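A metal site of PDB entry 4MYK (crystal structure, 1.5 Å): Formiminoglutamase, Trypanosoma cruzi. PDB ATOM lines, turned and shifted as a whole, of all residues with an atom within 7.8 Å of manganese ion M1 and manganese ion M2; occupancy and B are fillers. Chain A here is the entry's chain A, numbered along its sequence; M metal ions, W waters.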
ATOM      1  N   GLY A  42     -35.404 -20.080 -19.550  1.00  0.00           N
ATOM      2  CA  GLY A  42     -34.076 -20.514 -19.173  1.00  0.00           C
ATOM      3  C   GLY A  42     -33.878 -20.183 -17.708  1.00  0.00           C
ATOM      4  O   GLY A  42     -34.617 -20.650 -16.854  1.00  0.00           O
ATOM      5  N   CYS A  43     -32.885 -19.339 -17.418  1.00  0.00           N
ATOM      6  CA  CYS A  43     -32.527 -19.025 -16.035  1.00  0.00           C
ATOM      7  C   CYS A  43     -33.557 -18.152 -15.307  1.00  0.00           C
ATOM      8  O   CYS A  43     -33.543 -18.052 -14.072  1.00  0.00           O
ATOM      9  CB  CYS A  43     -31.138 -18.388 -15.977  1.00  0.00           C
ATOM     10  SG  CYS A  43     -30.355 -18.559 -14.374  1.00  0.00           S
ATOM     11  N   ASN A  46     -34.883 -20.299 -12.773  1.00  0.00           N
ATOM     12  CA  ASN A  46     -34.077 -20.499 -11.580  1.00  0.00           C
ATOM     13  C   ASN A  46     -33.683 -19.173 -10.918  1.00  0.00           C
ATOM     14  O   ASN A  46     -32.512 -18.924 -10.646  1.00  0.00           O
ATOM     15  CB  ASN A  46     -32.824 -21.307 -11.912  1.00  0.00           C
ATOM     16  CG  ASN A  46     -33.123 -22.515 -12.764  1.00  0.00           C
ATOM     17  OD1 ASN A  46     -33.915 -23.383 -12.373  1.00  0.00           O
ATOM     18  ND2 ASN A  46     -32.513 -22.595 -13.947  1.00  0.00           N
ATOM     19  N   GLY A 121     -33.398 -17.238 -23.841  1.00  0.00           N
ATOM     20  CA  GLY A 121     -32.897 -18.024 -22.717  1.00  0.00           C
ATOM     21  C   GLY A 121     -32.247 -19.360 -23.061  1.00  0.00           C
ATOM     22  O   GLY A 121     -32.339 -19.839 -24.178  1.00  0.00           O
ATOM     23  N   ASN A 122     -31.592 -19.961 -22.059  1.00  0.00           N
ATOM     24  CA  ASN A 122     -30.841 -21.222 -22.188  1.00  0.00           C
ATOM     25  C   ASN A 122     -31.549 -22.304 -23.003  1.00  0.00           C
ATOM     26  O   ASN A 122     -30.887 -23.145 -23.644  1.00  0.00           O
ATOM     27  CB  ASN A 122     -30.572 -21.832 -20.800  1.00  0.00           C
ATOM     28  CG  ASN A 122     -29.645 -20.978 -19.942  1.00  0.00           C
ATOM     29  OD1 ASN A 122     -28.640 -20.429 -20.409  1.00  0.00           O
ATOM     30  ND2 ASN A 122     -29.957 -20.893 -18.655  1.00  0.00           N
ATOM     31  N   ASP A 123     -32.871 -22.291 -22.960  1.00  0.00           N
ATOM     32  CA  ASP A 123     -33.681 -23.402 -23.474  1.00  0.00           C
ATOM     33  C   ASP A 123     -33.534 -23.640 -24.986  1.00  0.00           C
ATOM     34  O   ASP A 123     -33.778 -24.734 -25.475  1.00  0.00           O
ATOM     35  CB  ASP A 123     -35.135 -23.245 -23.056  1.00  0.00           C
ATOM     36  CG  ASP A 123     -35.343 -23.458 -21.558  1.00  0.00           C
ATOM     37  OD1 ASP A 123     -36.513 -23.428 -21.109  1.00  0.00           O
ATOM     38  OD2 ASP A 123     -34.350 -23.657 -20.831  1.00  0.00           O
ATOM     39  N   SER A 125     -30.948 -24.072 -26.455  1.00  0.00           N
ATOM     40  CA  SER A 125     -29.820 -24.969 -26.669  1.00  0.00           C
ATOM     41  C   SER A 125     -30.261 -26.390 -26.952  1.00  0.00           C
ATOM     42  O   SER A 125     -29.549 -27.139 -27.617  1.00  0.00           O
ATOM     43  CB  SER A 125     -28.893 -24.944 -25.457  1.00  0.00           C
ATOM     44  OG  SER A 125     -28.579 -23.611 -25.097  1.00  0.00           O
ATOM     45  N   ASN A 144     -20.937 -26.563 -22.848  1.00  0.00           N
ATOM     46  CA  ASN A 144     -21.778 -25.569 -22.200  1.00  0.00           C
ATOM     47  C   ASN A 144     -20.914 -24.641 -21.335  1.00  0.00           C
ATOM     48  O   ASN A 144     -20.468 -25.021 -20.241  1.00  0.00           O
ATOM     49  CB  ASN A 144     -22.883 -26.250 -21.366  1.00  0.00           C
ATOM     50  CG  ASN A 144     -23.842 -25.264 -20.678  1.00  0.00           C
ATOM     51  OD1 ASN A 144     -24.070 -24.156 -21.161  1.00  0.00           O
ATOM     52  ND2 ASN A 144     -24.399 -25.673 -19.548  1.00  0.00           N
ATOM     53  N   VAL A 145     -20.670 -23.436 -21.862  1.00  0.00           N
ATOM     54  CA  VAL A 145     -20.060 -22.343 -21.108  1.00  0.00           C
ATOM     55  C   VAL A 145     -21.149 -21.667 -20.281  1.00  0.00           C
ATOM     56  O   VAL A 145     -22.053 -21.010 -20.839  1.00  0.00           O
ATOM     57  CB  VAL A 145     -19.398 -21.282 -22.024  1.00  0.00           C
ATOM     58  CG1 VAL A 145     -18.716 -20.185 -21.180  1.00  0.00           C
ATOM     59  CG2 VAL A 145     -18.409 -21.951 -22.982  1.00  0.00           C
ATOM     60  N   ASP A 146     -21.087 -21.839 -18.962  1.00  0.00           N
ATOM     61  CA  ASP A 146     -22.204 -21.508 -18.119  1.00  0.00           C
ATOM     62  C   ASP A 146     -21.764 -21.573 -16.672  1.00  0.00           C
ATOM     63  O   ASP A 146     -21.105 -22.530 -16.276  1.00  0.00           O
ATOM     64  CB  ASP A 146     -23.314 -22.528 -18.373  1.00  0.00           C
ATOM     65  CG  ASP A 146     -24.644 -22.080 -17.852  1.00  0.00           C
ATOM     66  OD1 ASP A 146     -24.685 -21.079 -17.099  1.00  0.00           O
ATOM     67  OD2 ASP A 146     -25.637 -22.733 -18.189  1.00  0.00           O
ATOM     68  N   SER A 147     -22.096 -20.543 -15.897  1.00  0.00           N
ATOM     69  CA  SER A 147     -21.798 -20.532 -14.462  1.00  0.00           C
ATOM     70  C   SER A 147     -22.705 -21.517 -13.753  1.00  0.00           C
ATOM     71  O   SER A 147     -22.486 -21.877 -12.603  1.00  0.00           O
ATOM     72  CB  SER A 147     -21.942 -19.128 -13.872  1.00  0.00           C
ATOM     73  OG  SER A 147     -23.260 -18.640 -13.968  1.00  0.00           O
ATOM     74  N   HIS A 148     -23.746 -21.934 -14.463  1.00  0.00           N
ATOM     75  CA  HIS A 148     -24.745 -22.853 -13.944  1.00  0.00           C
ATOM     76  C   HIS A 148     -24.559 -24.241 -14.557  1.00  0.00           C
ATOM     77  O   HIS A 148     -24.114 -24.398 -15.697  1.00  0.00           O
ATOM     78  CB  HIS A 148     -26.175 -22.337 -14.215  1.00  0.00           C
ATOM     79  CG  HIS A 148     -26.446 -20.978 -13.634  1.00  0.00           C
ATOM     80  ND1 HIS A 148     -26.541 -19.849 -14.411  1.00  0.00           N
ATOM     81  CD2 HIS A 148     -26.616 -20.568 -12.359  1.00  0.00           C
ATOM     82  CE1 HIS A 148     -26.773 -18.801 -13.647  1.00  0.00           C
ATOM     83  NE2 HIS A 148     -26.819 -19.215 -12.396  1.00  0.00           N
ATOM     84  N   LEU A 149     -24.893 -25.241 -13.750  1.00  0.00           N
ATOM     85  CA  LEU A 149     -24.936 -26.617 -14.180  1.00  0.00           C
ATOM     86  C   LEU A 149     -26.286 -27.133 -13.697  1.00  0.00           C
ATOM     87  O   LEU A 149     -26.416 -27.676 -12.604  1.00  0.00           O
ATOM     88  CB  LEU A 149     -23.756 -27.372 -13.571  1.00  0.00           C
ATOM     89  CG  LEU A 149     -23.802 -28.860 -13.219  1.00  0.00           C
ATOM     90  CD1 LEU A 149     -24.622 -29.681 -14.208  1.00  0.00           C
ATOM     91  CD2 LEU A 149     -22.368 -29.385 -13.090  1.00  0.00           C
ATOM     92  N   ASP A 150     -27.305 -26.916 -14.531  1.00  0.00           N
ATOM     93  CA  ASP A 150     -28.696 -27.206 -14.194  1.00  0.00           C
ATOM     94  C   ASP A 150     -29.246 -28.289 -15.106  1.00  0.00           C
ATOM     95  O   ASP A 150     -29.492 -28.061 -16.294  1.00  0.00           O
ATOM     96  CB  ASP A 150     -29.533 -25.932 -14.296  1.00  0.00           C
ATOM     97  CG  ASP A 150     -30.964 -26.132 -13.848  1.00  0.00           C
ATOM     98  OD1 ASP A 150     -31.384 -27.297 -13.678  1.00  0.00           O
ATOM     99  OD2 ASP A 150     -31.669 -25.127 -13.663  1.00  0.00           O
ATOM    100  N   PRO A 165     -31.998 -27.685 -20.805  1.00  0.00           N
ATOM    101  CA  PRO A 165     -31.599 -28.069 -22.179  1.00  0.00           C
ATOM    102  C   PRO A 165     -30.567 -29.208 -22.291  1.00  0.00           C
ATOM    103  O   PRO A 165     -30.582 -29.948 -23.276  1.00  0.00           O
ATOM    104  CB  PRO A 165     -31.022 -26.772 -22.760  1.00  0.00           C
ATOM    105  CG  PRO A 165     -30.765 -25.882 -21.573  1.00  0.00           C
ATOM    106  CD  PRO A 165     -31.773 -26.261 -20.544  1.00  0.00           C
ATOM    107  N   PHE A 166     -29.681 -29.339 -21.308  1.00  0.00           N
ATOM    108  CA  PHE A 166     -28.582 -30.290 -21.455  1.00  0.00           C
ATOM    109  C   PHE A 166     -28.902 -31.636 -20.845  1.00  0.00           C
ATOM    110  O   PHE A 166     -28.282 -32.649 -21.168  1.00  0.00           O
ATOM    111  CB  PHE A 166     -27.280 -29.676 -20.948  1.00  0.00           C
ATOM    112  CG  PHE A 166     -26.839 -28.501 -21.770  1.00  0.00           C
ATOM    113  CD1 PHE A 166     -26.385 -28.678 -23.059  1.00  0.00           C
ATOM    114  CD2 PHE A 166     -26.956 -27.212 -21.276  1.00  0.00           C
ATOM    115  CE1 PHE A 166     -26.006 -27.619 -23.826  1.00  0.00           C
ATOM    116  CE2 PHE A 166     -26.578 -26.131 -22.065  1.00  0.00           C
ATOM    117  CZ  PHE A 166     -26.093 -26.339 -23.326  1.00  0.00           C
ATOM    118  N   GLU A 182     -19.014 -29.137 -19.254  1.00  0.00           N
ATOM    119  CA  GLU A 182     -19.552 -27.983 -18.547  1.00  0.00           C
ATOM    120  C   GLU A 182     -18.356 -27.097 -18.285  1.00  0.00           C
ATOM    121  O   GLU A 182     -17.426 -27.497 -17.586  1.00  0.00           O
ATOM    122  CB  GLU A 182     -20.189 -28.397 -17.224  1.00  0.00           C
ATOM    123  CG  GLU A 182     -21.377 -29.355 -17.364  1.00  0.00           C
ATOM    124  CD  GLU A 182     -22.690 -28.643 -17.643  1.00  0.00           C
ATOM    125  OE1 GLU A 182     -22.681 -27.496 -18.140  1.00  0.00           O
ATOM    126  OE2 GLU A 182     -23.753 -29.233 -17.357  1.00  0.00           O
ATOM    127  N   GLN A 189     -23.073 -22.708  -7.095  1.00  0.00           N
ATOM    128  CA  GLN A 189     -24.318 -22.680  -7.854  1.00  0.00           C
ATOM    129  C   GLN A 189     -24.607 -23.999  -8.533  1.00  0.00           C
ATOM    130  O   GLN A 189     -25.401 -24.037  -9.479  1.00  0.00           O
ATOM    131  CB  GLN A 189     -24.225 -21.635  -8.973  1.00  0.00           C
ATOM    132  CG  GLN A 189     -24.303 -20.210  -8.541  1.00  0.00           C
ATOM    133  CD  GLN A 189     -24.859 -19.337  -9.645  1.00  0.00           C
ATOM    134  OE1 GLN A 189     -25.820 -18.595  -9.433  1.00  0.00           O
ATOM    135  NE2 GLN A 189     -24.278 -19.450 -10.840  1.00  0.00           N
ATOM    136  N   SER A 234     -21.727 -23.556 -27.101  1.00  0.00           N
ATOM    137  CA  SER A 234     -22.888 -22.945 -26.441  1.00  0.00           C
ATOM    138  C   SER A 234     -22.425 -22.007 -25.332  1.00  0.00           C
ATOM    139  O   SER A 234     -21.851 -22.444 -24.324  1.00  0.00           O
ATOM    140  CB  SER A 234     -23.795 -24.032 -25.856  1.00  0.00           C
ATOM    141  OG  SER A 234     -25.026 -23.503 -25.390  1.00  0.00           O
ATOM    142  N   PHE A 235     -22.662 -20.714 -25.514  1.00  0.00           N
ATOM    143  CA  PHE A 235     -22.110 -19.713 -24.615  1.00  0.00           C
ATOM    144  C   PHE A 235     -23.160 -18.962 -23.820  1.00  0.00           C
ATOM    145  O   PHE A 235     -23.677 -17.948 -24.285  1.00  0.00           O
ATOM    146  CB  PHE A 235     -21.278 -18.697 -25.386  1.00  0.00           C
ATOM    147  CG  PHE A 235     -20.153 -18.105 -24.577  1.00  0.00           C
ATOM    148  CD1 PHE A 235     -20.375 -17.643 -23.295  1.00  0.00           C
ATOM    149  CD2 PHE A 235     -18.863 -18.017 -25.096  1.00  0.00           C
ATOM    150  CE1 PHE A 235     -19.353 -17.094 -22.552  1.00  0.00           C
ATOM    151  CE2 PHE A 235     -17.832 -17.472 -24.354  1.00  0.00           C
ATOM    152  CZ  PHE A 235     -18.079 -17.014 -23.085  1.00  0.00           C
ATOM    153  N   ASP A 236     -23.468 -19.438 -22.610  1.00  0.00           N
ATOM    154  CA  ASP A 236     -24.349 -18.693 -21.706  1.00  0.00           C
ATOM    155  C   ASP A 236     -23.571 -17.493 -21.200  1.00  0.00           C
ATOM    156  O   ASP A 236     -22.527 -17.659 -20.574  1.00  0.00           O
ATOM    157  CB  ASP A 236     -24.804 -19.566 -20.546  1.00  0.00           C
ATOM    158  CG  ASP A 236     -25.758 -18.853 -19.589  1.00  0.00           C
ATOM    159  OD1 ASP A 236     -25.764 -17.601 -19.516  1.00  0.00           O
ATOM    160  OD2 ASP A 236     -26.533 -19.549 -18.913  1.00  0.00           O
ATOM    161  N   VAL A 237     -24.059 -16.284 -21.466  1.00  0.00           N
ATOM    162  CA  VAL A 237     -23.288 -15.094 -21.122  1.00  0.00           C
ATOM    163  C   VAL A 237     -23.317 -14.743 -19.616  1.00  0.00           C
ATOM    164  O   VAL A 237     -22.563 -13.861 -19.165  1.00  0.00           O
ATOM    165  CB  VAL A 237     -23.637 -13.883 -22.021  1.00  0.00           C
ATOM    166  CG1 VAL A 237     -23.264 -14.167 -23.461  1.00  0.00           C
ATOM    167  CG2 VAL A 237     -25.106 -13.514 -21.912  1.00  0.00           C
ATOM    168  N   ASP A 238     -24.164 -15.429 -18.839  1.00  0.00           N
ATOM    169  CA  ASP A 238     -24.162 -15.250 -17.393  1.00  0.00           C
ATOM    170  C   ASP A 238     -23.011 -16.019 -16.740  1.00  0.00           C
ATOM    171  O   ASP A 238     -22.921 -16.138 -15.515  1.00  0.00           O
ATOM    172  CB  ASP A 238     -25.527 -15.566 -16.766  1.00  0.00           C
ATOM    173  CG  ASP A 238     -25.807 -17.058 -16.656  1.00  0.00           C
ATOM    174  OD1 ASP A 238     -24.862 -17.875 -16.717  1.00  0.00           O
ATOM    175  OD2 ASP A 238     -27.000 -17.422 -16.486  1.00  0.00           O
ATOM    176  N   SER A 239     -22.129 -16.553 -17.592  1.00  0.00           N
ATOM    177  CA  SER A 239     -20.865 -17.150 -17.145  1.00  0.00           C
ATOM    178  C   SER A 239     -19.768 -16.088 -16.998  1.00  0.00           C
ATOM    179  O   SER A 239     -18.666 -16.372 -16.526  1.00  0.00           O
ATOM    180  CB  SER A 239     -20.423 -18.201 -18.149  1.00  0.00           C
ATOM    181  OG  SER A 239     -20.133 -17.589 -19.390  1.00  0.00           O
ATOM    182  N   VAL A 248     -27.935  -9.718 -17.814  1.00  0.00           N
ATOM    183  CA  VAL A 248     -28.284 -11.121 -18.016  1.00  0.00           C
ATOM    184  C   VAL A 248     -29.349 -11.437 -16.987  1.00  0.00           C
ATOM    185  O   VAL A 248     -29.567 -10.640 -16.082  1.00  0.00           O
ATOM    186  CB  VAL A 248     -27.060 -12.078 -17.855  1.00  0.00           C
ATOM    187  CG1 VAL A 248     -25.938 -11.701 -18.809  1.00  0.00           C
ATOM    188  CG2 VAL A 248     -26.561 -12.095 -16.425  1.00  0.00           C
ATOM    189  N   CYS A 250     -29.525 -14.011 -14.841  1.00  0.00           N
ATOM    190  CA  CYS A 250     -28.911 -14.442 -13.595  1.00  0.00           C
ATOM    191  C   CYS A 250     -27.498 -13.889 -13.486  1.00  0.00           C
ATOM    192  O   CYS A 250     -26.534 -14.580 -13.778  1.00  0.00           O
ATOM    193  CB  CYS A 250     -28.871 -15.972 -13.528  1.00  0.00           C
ATOM    194  SG  CYS A 250     -30.508 -16.758 -13.433  1.00  0.00           S
ATOM    195  N   SER A 280     -26.624 -17.348 -25.018  1.00  0.00           N
ATOM    196  CA  SER A 280     -27.854 -17.353 -24.226  1.00  0.00           C
ATOM    197  C   SER A 280     -27.833 -16.353 -23.092  1.00  0.00           C
ATOM    198  O   SER A 280     -26.771 -15.996 -22.601  1.00  0.00           O
ATOM    199  CB  SER A 280     -28.085 -18.747 -23.631  1.00  0.00           C
ATOM    200  OG  SER A 280     -28.587 -19.633 -24.592  1.00  0.00           O
ATOM    201  N   GLU A 281     -29.026 -15.920 -22.688  1.00  0.00           N
ATOM    202  CA  GLU A 281     -29.268 -15.199 -21.434  1.00  0.00           C
ATOM    203  C   GLU A 281     -29.047 -13.672 -21.459  1.00  0.00           C
ATOM    204  O   GLU A 281     -29.133 -13.013 -20.433  1.00  0.00           O
ATOM    205  CB  GLU A 281     -28.533 -15.868 -20.262  1.00  0.00           C
ATOM    206  CG  GLU A 281     -29.019 -17.306 -19.963  1.00  0.00           C
ATOM    207  CD  GLU A 281     -30.454 -17.325 -19.463  1.00  0.00           C
ATOM    208  OE1 GLU A 281     -30.876 -16.310 -18.862  1.00  0.00           O
ATOM    209  OE2 GLU A 281     -31.160 -18.335 -19.658  1.00  0.00           O
HETATM  210 MN    MN M   1     -26.296 -19.673 -16.673  1.00  0.00          MN
HETATM  211 MN    MN M   2     -27.421 -21.695 -18.429  1.00  0.00          MN
HETATM  212  O   HOH W   1     -28.370 -20.887 -16.697  1.00  0.00           O
HETATM  213  O   HOH W   2     -27.667 -23.734 -20.038  1.00  0.00           O
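Within 4 Å of manganese ion M1: Asp 146, His 148, Asp 236 and Asp 238.
The nearest printed residue that does not touch manganese ion M1 is Ser 147 (4.2 Å).
Manganese ion M2 is bound by OD2 of Asp 146 (2.1 Å), water W1 (2.1 Å), OD2 of Asp 236 (2.4 Å), water W2 (2.6 Å), OD1 of Asn 122 (2.6 Å) and ND2 of Asn 122 (2.7 Å).
Manganese ion M2 has six donor atoms within binding distance.
Manganese ion M1 is bound by OD1 of Asp 146 (2.2 Å), OD2 of Asp 236 (2.3 Å), ND1 of His 148 (2.3 Å), OD1 of Asp 238 (2.3 Å), OD2 of Asp 238 (2.4 Å) and water W1 (2.4 Å).
Manganese ion M1 has six donor atoms within binding distance.
Along chain A the residues within 4 Å of manganese ion M2 span positions 122 to 236.
The nearest printed residue that does not touch manganese ion M2 is His 148 (4.4 Å).
The side-chain hydroxyl (OG) of Ser 239 lies within hydrogen-bond range of the backbone carbonyl oxygen (O) of Asp 236 (2.7 Å).
OG of Ser 125 lies within hydrogen-bond range of O of Asn 122, at 2.8 Å.
The side-chain sulfur (SG) of Cys 250 forms a disulfide with the side-chain sulfur (SG) of Cys 43 (2.0 Å).
The backbone carbonyl oxygen (O) of Asp 238 sits at hydrogen-bond distance from the side-chain hydroxyl (OG) of Ser 147 (3.0 Å).
The backbone NH of Asn 122 lies within hydrogen-bond range of the side-chain carboxylate of Glu 281.
The side-chain carboxylate (OD2) of Asp 146 sits close to the side-chain amide nitrogen (ND2) of Asn 144.
NE2 of His 148 sits at hydrogen-bond distance from NE2 of Gln 189 (3.0 Å).
N of Asp 236 lies within hydrogen-bond range of O of Val 145 (2.8 Å).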
